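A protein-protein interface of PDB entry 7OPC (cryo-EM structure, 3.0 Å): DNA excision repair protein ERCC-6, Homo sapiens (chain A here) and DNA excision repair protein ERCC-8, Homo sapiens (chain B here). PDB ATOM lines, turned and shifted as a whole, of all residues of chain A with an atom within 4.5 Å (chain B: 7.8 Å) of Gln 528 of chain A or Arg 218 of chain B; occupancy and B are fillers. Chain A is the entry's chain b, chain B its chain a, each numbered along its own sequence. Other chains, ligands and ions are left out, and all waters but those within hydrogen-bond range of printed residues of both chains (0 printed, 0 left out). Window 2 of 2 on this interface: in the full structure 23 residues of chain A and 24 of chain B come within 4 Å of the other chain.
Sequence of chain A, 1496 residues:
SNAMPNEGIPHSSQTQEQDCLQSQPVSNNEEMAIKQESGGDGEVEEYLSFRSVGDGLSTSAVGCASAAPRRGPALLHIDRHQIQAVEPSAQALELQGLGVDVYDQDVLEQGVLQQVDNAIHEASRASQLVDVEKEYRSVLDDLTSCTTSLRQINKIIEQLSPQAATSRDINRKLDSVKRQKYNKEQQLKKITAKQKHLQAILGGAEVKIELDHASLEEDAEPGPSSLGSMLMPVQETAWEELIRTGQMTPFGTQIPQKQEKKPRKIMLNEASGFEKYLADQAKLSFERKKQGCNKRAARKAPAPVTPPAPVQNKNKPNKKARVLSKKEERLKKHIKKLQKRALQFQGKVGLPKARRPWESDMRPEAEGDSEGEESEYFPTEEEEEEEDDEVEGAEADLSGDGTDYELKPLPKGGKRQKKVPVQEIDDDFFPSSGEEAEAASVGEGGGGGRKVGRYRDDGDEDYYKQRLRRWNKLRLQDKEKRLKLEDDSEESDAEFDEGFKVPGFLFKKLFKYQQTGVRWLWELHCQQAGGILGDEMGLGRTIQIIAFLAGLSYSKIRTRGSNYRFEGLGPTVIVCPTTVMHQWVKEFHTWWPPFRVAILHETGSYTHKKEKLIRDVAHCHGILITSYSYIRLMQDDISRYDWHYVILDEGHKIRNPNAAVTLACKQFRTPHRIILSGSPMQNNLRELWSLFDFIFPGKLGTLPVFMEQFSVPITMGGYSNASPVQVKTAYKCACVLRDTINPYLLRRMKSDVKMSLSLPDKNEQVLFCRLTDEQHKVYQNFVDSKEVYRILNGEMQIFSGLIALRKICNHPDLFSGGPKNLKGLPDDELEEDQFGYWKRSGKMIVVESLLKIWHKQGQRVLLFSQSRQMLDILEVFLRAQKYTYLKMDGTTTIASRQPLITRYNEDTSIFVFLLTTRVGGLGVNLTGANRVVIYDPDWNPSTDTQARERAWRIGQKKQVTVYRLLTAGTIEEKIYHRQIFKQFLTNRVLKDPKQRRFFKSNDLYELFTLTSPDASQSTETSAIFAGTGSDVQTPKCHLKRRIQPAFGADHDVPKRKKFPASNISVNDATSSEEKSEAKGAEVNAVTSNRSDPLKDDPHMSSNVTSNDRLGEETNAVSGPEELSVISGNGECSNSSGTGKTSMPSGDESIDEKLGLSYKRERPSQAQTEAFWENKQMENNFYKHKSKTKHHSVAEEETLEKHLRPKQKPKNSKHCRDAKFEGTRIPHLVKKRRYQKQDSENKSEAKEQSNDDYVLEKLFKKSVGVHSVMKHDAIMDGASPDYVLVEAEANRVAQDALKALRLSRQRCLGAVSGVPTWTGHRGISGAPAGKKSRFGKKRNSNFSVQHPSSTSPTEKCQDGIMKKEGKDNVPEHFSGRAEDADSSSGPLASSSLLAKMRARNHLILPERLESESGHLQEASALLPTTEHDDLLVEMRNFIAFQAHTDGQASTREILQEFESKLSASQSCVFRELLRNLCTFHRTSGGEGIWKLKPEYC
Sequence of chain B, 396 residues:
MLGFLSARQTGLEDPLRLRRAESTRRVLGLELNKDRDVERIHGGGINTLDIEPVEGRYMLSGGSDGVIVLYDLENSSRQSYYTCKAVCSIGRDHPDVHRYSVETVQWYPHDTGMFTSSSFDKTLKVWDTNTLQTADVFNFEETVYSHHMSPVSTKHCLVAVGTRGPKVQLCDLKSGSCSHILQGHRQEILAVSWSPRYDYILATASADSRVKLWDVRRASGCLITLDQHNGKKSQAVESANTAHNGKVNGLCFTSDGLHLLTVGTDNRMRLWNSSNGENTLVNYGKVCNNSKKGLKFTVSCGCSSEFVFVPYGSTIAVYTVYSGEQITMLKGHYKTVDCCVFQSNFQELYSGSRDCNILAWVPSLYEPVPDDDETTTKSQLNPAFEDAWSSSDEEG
OE1 of Gln 528 of chain A sits at hydrogen-bond distance from NE of Arg 218 of chain B (2.8 Å). The backbone NH of Ala 219 of chain B sits at hydrogen-bond distance from the backbone carbonyl oxygen of Gln 528 of chain A.
The backbone carbonyl oxygen of Leu 524 of chain A is in hydrogen-bond range of the backbone NH of Ala 529 of chain A. The side-chain carboxylate (OD1) of Asp 215 of chain B lies within salt-bridge range of the guanidinium group (NE) of Arg 217 of chain B, 3.5 Å away. The side-chain carboxylate (OD2) of Asp 215 of chain B is in salt-bridge range of the guanidinium group (NH2) of Arg 218 of chain B.
Gln 527 of chain A touches Arg 217 of chain B (O to O, 3.9 Å). Arg 218 of chain B touches Gln 527 of chain A (CA to O, 3.5 Å). Ala 529 of chain A touches Ala 219 of chain B (CA to CB, 3.9 Å). Pro 671 of chain A touches Ser 220 of chain B (CB to CB, 3.9 Å). His 180 of chain B touches Phe 696 of chain A (CE1 to CE1, 3.3 Å). Phe 696 of chain A touches Arg 217 of chain B. Ala 219 of chain B touches Phe 696 of chain A.
Arg 218 of chain B touches two residues of chain A. Of the printed residues of chain B, Gln 527 of chain A touches Arg 217 and Arg 218. Printed residues of chain B within 4 Å of Pro 671 of chain A: Ser 220. Cys 222 of chain B touches none of the printed residues of chain A. Leu 524 of chain A touches none of the printed residues of chain B. The nearest residue of chain B that does not touch Gln 528 of chain A is Arg 217 of chain B (4.5 Å). The nearest residue of chain A that does not touch Arg 218 of chain B is Phe 696 of chain A (4.1 Å). The nearest printed residue of chain A that does not touch Ser 220 of chain B is Gln 528 of chain A (4.9 Å).
Hydrophobic or aromatic side chains of chain A within 4 Å of the printed part of chain B: Pro 671 and Phe 696. Hydrophobic or aromatic side chains of chain B that line the printed part of chain A: His 180 and Ala 219. Along chain B the printed residues that touch a printed residue of chain A span positions 180 to 220. Among the printed residues, 9 pairs touch across the chains.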
ATOM      1  N   LEU A 524      18.656 -37.148 -16.905  1.00  0.00           N
ATOM      2  CA  LEU A 524      19.682 -36.581 -17.758  1.00  0.00           C
ATOM      3  C   LEU A 524      19.246 -36.610 -19.188  1.00  0.00           C
ATOM      4  O   LEU A 524      19.347 -35.608 -19.880  1.00  0.00           O
ATOM      5  CB  LEU A 524      20.988 -37.323 -17.633  1.00  0.00           C
ATOM      6  CG  LEU A 524      21.787 -37.132 -16.382  1.00  0.00           C
ATOM      7  CD1 LEU A 524      22.877 -38.077 -16.415  1.00  0.00           C
ATOM      8  CD2 LEU A 524      22.314 -35.781 -16.250  1.00  0.00           C
ATOM      9  N   HIS A 525      18.706 -37.727 -19.636  1.00  0.00           N
ATOM     10  CA  HIS A 525      18.262 -37.805 -21.012  1.00  0.00           C
ATOM     11  C   HIS A 525      17.288 -36.724 -21.322  1.00  0.00           C
ATOM     12  O   HIS A 525      17.239 -36.226 -22.439  1.00  0.00           O
ATOM     13  CB  HIS A 525      17.616 -39.135 -21.257  1.00  0.00           C
ATOM     14  CG  HIS A 525      17.031 -39.280 -22.613  1.00  0.00           C
ATOM     15  ND1 HIS A 525      17.762 -39.697 -23.690  1.00  0.00           N
ATOM     16  CD2 HIS A 525      15.771 -39.117 -23.060  1.00  0.00           C
ATOM     17  CE1 HIS A 525      16.985 -39.770 -24.750  1.00  0.00           C
ATOM     18  NE2 HIS A 525      15.770 -39.428 -24.393  1.00  0.00           N
ATOM     19  N   CYS A 526      16.464 -36.381 -20.360  1.00  0.00           N
ATOM     20  CA  CYS A 526      15.545 -35.289 -20.571  1.00  0.00           C
ATOM     21  C   CYS A 526      16.280 -33.978 -20.693  1.00  0.00           C
ATOM     22  O   CYS A 526      16.001 -33.193 -21.594  1.00  0.00           O
ATOM     23  CB  CYS A 526      14.543 -35.257 -19.445  1.00  0.00           C
ATOM     24  SG  CYS A 526      13.436 -36.634 -19.471  1.00  0.00           S
ATOM     25  N   GLN A 527      17.235 -33.727 -19.823  1.00  0.00           N
ATOM     26  CA  GLN A 527      18.032 -32.528 -19.967  1.00  0.00           C
ATOM     27  C   GLN A 527      18.851 -32.533 -21.225  1.00  0.00           C
ATOM     28  O   GLN A 527      19.189 -31.469 -21.709  1.00  0.00           O
ATOM     29  CB  GLN A 527      18.968 -32.404 -18.811  1.00  0.00           C
ATOM     30  CG  GLN A 527      18.379 -31.791 -17.677  1.00  0.00           C
ATOM     31  CD  GLN A 527      18.980 -32.316 -16.441  1.00  0.00           C
ATOM     32  OE1 GLN A 527      18.510 -33.293 -15.901  1.00  0.00           O
ATOM     33  NE2 GLN A 527      20.025 -31.674 -15.964  1.00  0.00           N
ATOM     34  N   GLN A 528      19.138 -33.692 -21.792  1.00  0.00           N
ATOM     35  CA  GLN A 528      20.132 -33.879 -22.847  1.00  0.00           C
ATOM     36  C   GLN A 528      21.518 -33.541 -22.351  1.00  0.00           C
ATOM     37  O   GLN A 528      22.251 -32.791 -22.965  1.00  0.00           O
ATOM     38  CB  GLN A 528      19.806 -33.073 -24.081  1.00  0.00           C
ATOM     39  CG  GLN A 528      18.567 -33.470 -24.681  1.00  0.00           C
ATOM     40  CD  GLN A 528      18.325 -32.769 -25.925  1.00  0.00           C
ATOM     41  OE1 GLN A 528      17.665 -31.760 -25.931  1.00  0.00           O
ATOM     42  NE2 GLN A 528      18.813 -33.301 -27.013  1.00  0.00           N
ATOM     43  N   ALA A 529      21.881 -34.120 -21.231  1.00  0.00           N
ATOM     44  CA  ALA A 529      23.186 -33.962 -20.640  1.00  0.00           C
ATOM     45  C   ALA A 529      23.720 -35.334 -20.332  1.00  0.00           C
ATOM     46  O   ALA A 529      23.013 -36.319 -20.442  1.00  0.00           O
ATOM     47  CB  ALA A 529      23.133 -33.129 -19.391  1.00  0.00           C
ATOM     48  N   PRO A 671      24.478 -35.559 -27.231  1.00  0.00           N
ATOM     49  CA  PRO A 671      24.591 -35.143 -25.851  1.00  0.00           C
ATOM     50  C   PRO A 671      24.503 -36.241 -24.870  1.00  0.00           C
ATOM     51  O   PRO A 671      24.753 -36.018 -23.698  1.00  0.00           O
ATOM     52  CB  PRO A 671      23.416 -34.217 -25.688  1.00  0.00           C
ATOM     53  CG  PRO A 671      22.627 -34.488 -26.685  1.00  0.00           C
ATOM     54  CD  PRO A 671      23.348 -34.890 -27.820  1.00  0.00           C
ATOM     55  N   HIS A 672      24.108 -37.412 -25.279  1.00  0.00           N
ATOM     56  CA  HIS A 672      23.881 -38.491 -24.359  1.00  0.00           C
ATOM     57  C   HIS A 672      25.154 -39.262 -24.306  1.00  0.00           C
ATOM     58  O   HIS A 672      25.331 -40.291 -24.929  1.00  0.00           O
ATOM     59  CB  HIS A 672      22.720 -39.332 -24.801  1.00  0.00           C
ATOM     60  CG  HIS A 672      21.499 -38.543 -25.077  1.00  0.00           C
ATOM     61  ND1 HIS A 672      20.689 -38.056 -24.095  1.00  0.00           N
ATOM     62  CD2 HIS A 672      20.995 -38.106 -26.238  1.00  0.00           C
ATOM     63  CE1 HIS A 672      19.709 -37.378 -24.648  1.00  0.00           C
ATOM     64  NE2 HIS A 672      19.873 -37.396 -25.949  1.00  0.00           N
ATOM     65  N   PHE A 696      29.938 -33.367 -20.452  1.00  0.00           N
ATOM     66  CA  PHE A 696      29.236 -32.103 -20.473  1.00  0.00           C
ATOM     67  C   PHE A 696      30.240 -31.044 -20.867  1.00  0.00           C
ATOM     68  O   PHE A 696      30.793 -30.372 -20.007  1.00  0.00           O
ATOM     69  CB  PHE A 696      28.655 -31.797 -19.110  1.00  0.00           C
ATOM     70  CG  PHE A 696      27.660 -30.755 -19.145  1.00  0.00           C
ATOM     71  CD1 PHE A 696      28.045 -29.524 -19.361  1.00  0.00           C
ATOM     72  CD2 PHE A 696      26.343 -31.001 -19.194  1.00  0.00           C
ATOM     73  CE1 PHE A 696      27.218 -28.576 -19.455  1.00  0.00           C
ATOM     74  CE2 PHE A 696      25.502 -29.984 -19.272  1.00  0.00           C
ATOM     75  CZ  PHE A 696      25.950 -28.789 -19.428  1.00  0.00           C
ATOM     76  N   HIS B 180      30.636 -22.686 -15.826  1.00  0.00           N
ATOM     77  CA  HIS B 180      29.857 -23.092 -16.982  1.00  0.00           C
ATOM     78  C   HIS B 180      29.926 -22.034 -18.060  1.00  0.00           C
ATOM     79  O   HIS B 180      29.768 -20.843 -17.785  1.00  0.00           O
ATOM     80  CB  HIS B 180      28.408 -23.320 -16.586  1.00  0.00           C
ATOM     81  CG  HIS B 180      27.564 -23.826 -17.704  1.00  0.00           C
ATOM     82  ND1 HIS B 180      27.393 -25.164 -17.955  1.00  0.00           N
ATOM     83  CD2 HIS B 180      26.888 -23.175 -18.675  1.00  0.00           C
ATOM     84  CE1 HIS B 180      26.617 -25.319 -19.008  1.00  0.00           C
ATOM     85  NE2 HIS B 180      26.295 -24.126 -19.466  1.00  0.00           N
ATOM     86  N   ILE B 181      30.170 -22.465 -19.287  1.00  0.00           N
ATOM     87  CA  ILE B 181      30.280 -21.559 -20.413  1.00  0.00           C
ATOM     88  C   ILE B 181      29.565 -22.143 -21.614  1.00  0.00           C
ATOM     89  O   ILE B 181      29.585 -23.355 -21.838  1.00  0.00           O
ATOM     90  CB  ILE B 181      31.738 -21.257 -20.769  1.00  0.00           C
ATOM     91  CG1 ILE B 181      32.513 -22.563 -20.817  1.00  0.00           C
ATOM     92  CG2 ILE B 181      32.346 -20.278 -19.796  1.00  0.00           C
ATOM     93  CD1 ILE B 181      33.785 -22.433 -21.473  1.00  0.00           C
ATOM     94  N   LEU B 182      28.931 -21.278 -22.374  1.00  0.00           N
ATOM     95  CA  LEU B 182      28.312 -21.647 -23.632  1.00  0.00           C
ATOM     96  C   LEU B 182      29.259 -21.194 -24.727  1.00  0.00           C
ATOM     97  O   LEU B 182      29.674 -20.032 -24.761  1.00  0.00           O
ATOM     98  CB  LEU B 182      26.935 -21.019 -23.783  1.00  0.00           C
ATOM     99  CG  LEU B 182      26.026 -21.158 -22.571  1.00  0.00           C
ATOM    100  CD1 LEU B 182      24.942 -20.127 -22.624  1.00  0.00           C
ATOM    101  CD2 LEU B 182      25.454 -22.543 -22.534  1.00  0.00           C
ATOM    102  N   TYR B 200      14.894 -22.382 -19.069  1.00  0.00           N
ATOM    103  CA  TYR B 200      16.295 -22.587 -19.397  1.00  0.00           C
ATOM    104  C   TYR B 200      16.660 -22.150 -20.801  1.00  0.00           C
ATOM    105  O   TYR B 200      17.719 -22.547 -21.290  1.00  0.00           O
ATOM    106  CB  TYR B 200      16.655 -24.054 -19.213  1.00  0.00           C
ATOM    107  CG  TYR B 200      16.561 -24.498 -17.786  1.00  0.00           C
ATOM    108  CD1 TYR B 200      17.621 -24.317 -16.919  1.00  0.00           C
ATOM    109  CD2 TYR B 200      15.422 -25.108 -17.306  1.00  0.00           C
ATOM    110  CE1 TYR B 200      17.551 -24.735 -15.623  1.00  0.00           C
ATOM    111  CE2 TYR B 200      15.336 -25.516 -16.001  1.00  0.00           C
ATOM    112  CZ  TYR B 200      16.403 -25.324 -15.162  1.00  0.00           C
ATOM    113  OH  TYR B 200      16.327 -25.736 -13.855  1.00  0.00           O
ATOM    114  N   ILE B 201      15.830 -21.364 -21.472  1.00  0.00           N
ATOM    115  CA  ILE B 201      16.187 -20.857 -22.788  1.00  0.00           C
ATOM    116  C   ILE B 201      16.845 -19.497 -22.616  1.00  0.00           C
ATOM    117  O   ILE B 201      16.315 -18.618 -21.933  1.00  0.00           O
ATOM    118  CB  ILE B 201      14.978 -20.777 -23.724  1.00  0.00           C
ATOM    119  CG1 ILE B 201      14.399 -22.172 -23.960  1.00  0.00           C
ATOM    120  CG2 ILE B 201      15.389 -20.138 -25.047  1.00  0.00           C
ATOM    121  CD1 ILE B 201      15.289 -23.134 -24.691  1.00  0.00           C
ATOM    122  N   TRP B 214      19.939 -20.803 -26.612  1.00  0.00           N
ATOM    123  CA  TRP B 214      20.526 -21.943 -25.940  1.00  0.00           C
ATOM    124  C   TRP B 214      19.522 -22.549 -24.987  1.00  0.00           C
ATOM    125  O   TRP B 214      18.713 -21.848 -24.393  1.00  0.00           O
ATOM    126  CB  TRP B 214      21.746 -21.553 -25.119  1.00  0.00           C
ATOM    127  CG  TRP B 214      22.708 -20.713 -25.818  1.00  0.00           C
ATOM    128  CD1 TRP B 214      22.631 -19.381 -26.024  1.00  0.00           C
ATOM    129  CD2 TRP B 214      23.922 -21.143 -26.406  1.00  0.00           C
ATOM    130  NE1 TRP B 214      23.722 -18.947 -26.716  1.00  0.00           N
ATOM    131  CE2 TRP B 214      24.535 -20.018 -26.961  1.00  0.00           C
ATOM    132  CE3 TRP B 214      24.555 -22.378 -26.515  1.00  0.00           C
ATOM    133  CZ2 TRP B 214      25.746 -20.086 -27.611  1.00  0.00           C
ATOM    134  CZ3 TRP B 214      25.747 -22.444 -27.158  1.00  0.00           C
ATOM    135  CH2 TRP B 214      26.336 -21.309 -27.701  1.00  0.00           C
ATOM    136  N   ASP B 215      19.629 -23.855 -24.803  1.00  0.00           N
ATOM    137  CA  ASP B 215      19.006 -24.560 -23.693  1.00  0.00           C
ATOM    138  C   ASP B 215      20.168 -24.874 -22.768  1.00  0.00           C
ATOM    139  O   ASP B 215      20.899 -25.836 -22.988  1.00  0.00           O
ATOM    140  CB  ASP B 215      18.283 -25.806 -24.154  1.00  0.00           C
ATOM    141  CG  ASP B 215      17.621 -26.555 -23.020  1.00  0.00           C
ATOM    142  OD1 ASP B 215      17.862 -26.227 -21.846  1.00  0.00           O
ATOM    143  OD2 ASP B 215      16.851 -27.490 -23.309  1.00  0.00           O
ATOM    144  N   VAL B 216      20.360 -24.044 -21.744  1.00  0.00           N
ATOM    145  CA  VAL B 216      21.555 -24.164 -20.928  1.00  0.00           C
ATOM    146  C   VAL B 216      21.615 -25.498 -20.205  1.00  0.00           C
ATOM    147  O   VAL B 216      22.698 -25.942 -19.824  1.00  0.00           O
ATOM    148  CB  VAL B 216      21.649 -22.994 -19.938  1.00  0.00           C
ATOM    149  CG1 VAL B 216      21.608 -21.676 -20.676  1.00  0.00           C
ATOM    150  CG2 VAL B 216      20.544 -23.055 -18.911  1.00  0.00           C
ATOM    151  N   ARG B 217      20.477 -26.152 -20.000  1.00  0.00           N
ATOM    152  CA  ARG B 217      20.506 -27.514 -19.490  1.00  0.00           C
ATOM    153  C   ARG B 217      21.222 -28.419 -20.465  1.00  0.00           C
ATOM    154  O   ARG B 217      21.956 -29.327 -20.070  1.00  0.00           O
ATOM    155  CB  ARG B 217      19.091 -28.042 -19.313  1.00  0.00           C
ATOM    156  CG  ARG B 217      18.355 -27.571 -18.107  1.00  0.00           C
ATOM    157  CD  ARG B 217      16.964 -28.184 -18.063  1.00  0.00           C
ATOM    158  NE  ARG B 217      16.217 -27.950 -19.296  1.00  0.00           N
ATOM    159  CZ  ARG B 217      15.095 -28.575 -19.633  1.00  0.00           C
ATOM    160  NH1 ARG B 217      14.562 -29.494 -18.838  1.00  0.00           N
ATOM    161  NH2 ARG B 217      14.504 -28.285 -20.782  1.00  0.00           N
ATOM    162  N   ARG B 218      20.990 -28.186 -21.744  1.00  0.00           N
ATOM    163  CA  ARG B 218      21.462 -29.056 -22.796  1.00  0.00           C
ATOM    164  C   ARG B 218      22.978 -28.985 -22.883  1.00  0.00           C
ATOM    165  O   ARG B 218      23.587 -27.946 -22.626  1.00  0.00           O
ATOM    166  CB  ARG B 218      20.813 -28.626 -24.103  1.00  0.00           C
ATOM    167  CG  ARG B 218      21.001 -29.569 -25.244  1.00  0.00           C
ATOM    168  CD  ARG B 218      19.992 -29.374 -26.384  1.00  0.00           C
ATOM    169  NE  ARG B 218      18.606 -29.172 -25.958  1.00  0.00           N
ATOM    170  CZ  ARG B 218      17.565 -29.141 -26.786  1.00  0.00           C
ATOM    171  NH1 ARG B 218      17.731 -29.325 -28.090  1.00  0.00           N
ATOM    172  NH2 ARG B 218      16.345 -28.945 -26.307  1.00  0.00           N
ATOM    173  N   ALA B 219      23.589 -30.101 -23.260  1.00  0.00           N
ATOM    174  CA  ALA B 219      25.037 -30.213 -23.340  1.00  0.00           C
ATOM    175  C   ALA B 219      25.520 -30.251 -24.781  1.00  0.00           C
ATOM    176  O   ALA B 219      26.597 -30.776 -25.056  1.00  0.00           O
ATOM    177  CB  ALA B 219      25.508 -31.467 -22.610  1.00  0.00           C
ATOM    178  N   SER B 220      24.756 -29.665 -25.706  1.00  0.00           N
ATOM    179  CA  SER B 220      24.993 -29.894 -27.126  1.00  0.00           C
ATOM    180  C   SER B 220      24.929 -28.617 -27.941  1.00  0.00           C
ATOM    181  O   SER B 220      24.603 -28.660 -29.131  1.00  0.00           O
ATOM    182  CB  SER B 220      23.979 -30.883 -27.687  1.00  0.00           C
ATOM    183  OG  SER B 220      22.674 -30.339 -27.655  1.00  0.00           O
ATOM    184  N   GLY B 221      25.247 -27.484 -27.350  1.00  0.00           N
ATOM    185  CA  GLY B 221      25.338 -26.275 -28.130  1.00  0.00           C
ATOM    186  C   GLY B 221      23.988 -25.628 -28.370  1.00  0.00           C
ATOM    187  O   GLY B 221      22.954 -26.026 -27.831  1.00  0.00           O
ATOM    188  N   CYS B 222      24.013 -24.605 -29.215  1.00  0.00           N
ATOM    189  CA  CYS B 222      22.848 -23.759 -29.412  1.00  0.00           C
ATOM    190  C   CYS B 222      21.698 -24.543 -30.017  1.00  0.00           C
ATOM    191  O   CYS B 222      21.903 -25.492 -30.773  1.00  0.00           O
ATOM    192  CB  CYS B 222      23.199 -22.585 -30.318  1.00  0.00           C
ATOM    193  SG  CYS B 222      23.611 -23.014 -32.014  1.00  0.00           S
ATOM    194  N   LEU B 223      20.479 -24.165 -29.639  1.00  0.00           N
ATOM    195  CA  LEU B 223      19.297 -24.703 -30.296  1.00  0.00           C
ATOM    196  C   LEU B 223      19.178 -24.180 -31.710  1.00  0.00           C
ATOM    197  O   LEU B 223      19.029 -24.947 -32.666  1.00  0.00           O
ATOM    198  CB  LEU B 223      18.050 -24.304 -29.532  1.00  0.00           C
ATOM    199  CG  LEU B 223      17.914 -24.878 -28.149  1.00  0.00           C
ATOM    200  CD1 LEU B 223      16.856 -24.124 -27.429  1.00  0.00           C
ATOM    201  CD2 LEU B 223      17.544 -26.294 -28.245  1.00  0.00           C
ATOM    202  N   ILE B 224      19.213 -22.866 -31.851  1.00  0.00           N
ATOM    203  CA  ILE B 224      18.827 -22.186 -33.071  1.00  0.00           C
ATOM    204  C   ILE B 224      19.836 -21.087 -33.313  1.00  0.00           C
ATOM    205  O   ILE B 224      20.320 -20.460 -32.368  1.00  0.00           O
ATOM    206  CB  ILE B 224      17.413 -21.587 -32.956  1.00  0.00           C
ATOM    207  CG1 ILE B 224      16.377 -22.688 -32.744  1.00  0.00           C
ATOM    208  CG2 ILE B 224      17.076 -20.803 -34.213  1.00  0.00           C
ATOM    209  CD1 ILE B 224      15.016 -22.198 -32.354  1.00  0.00           C
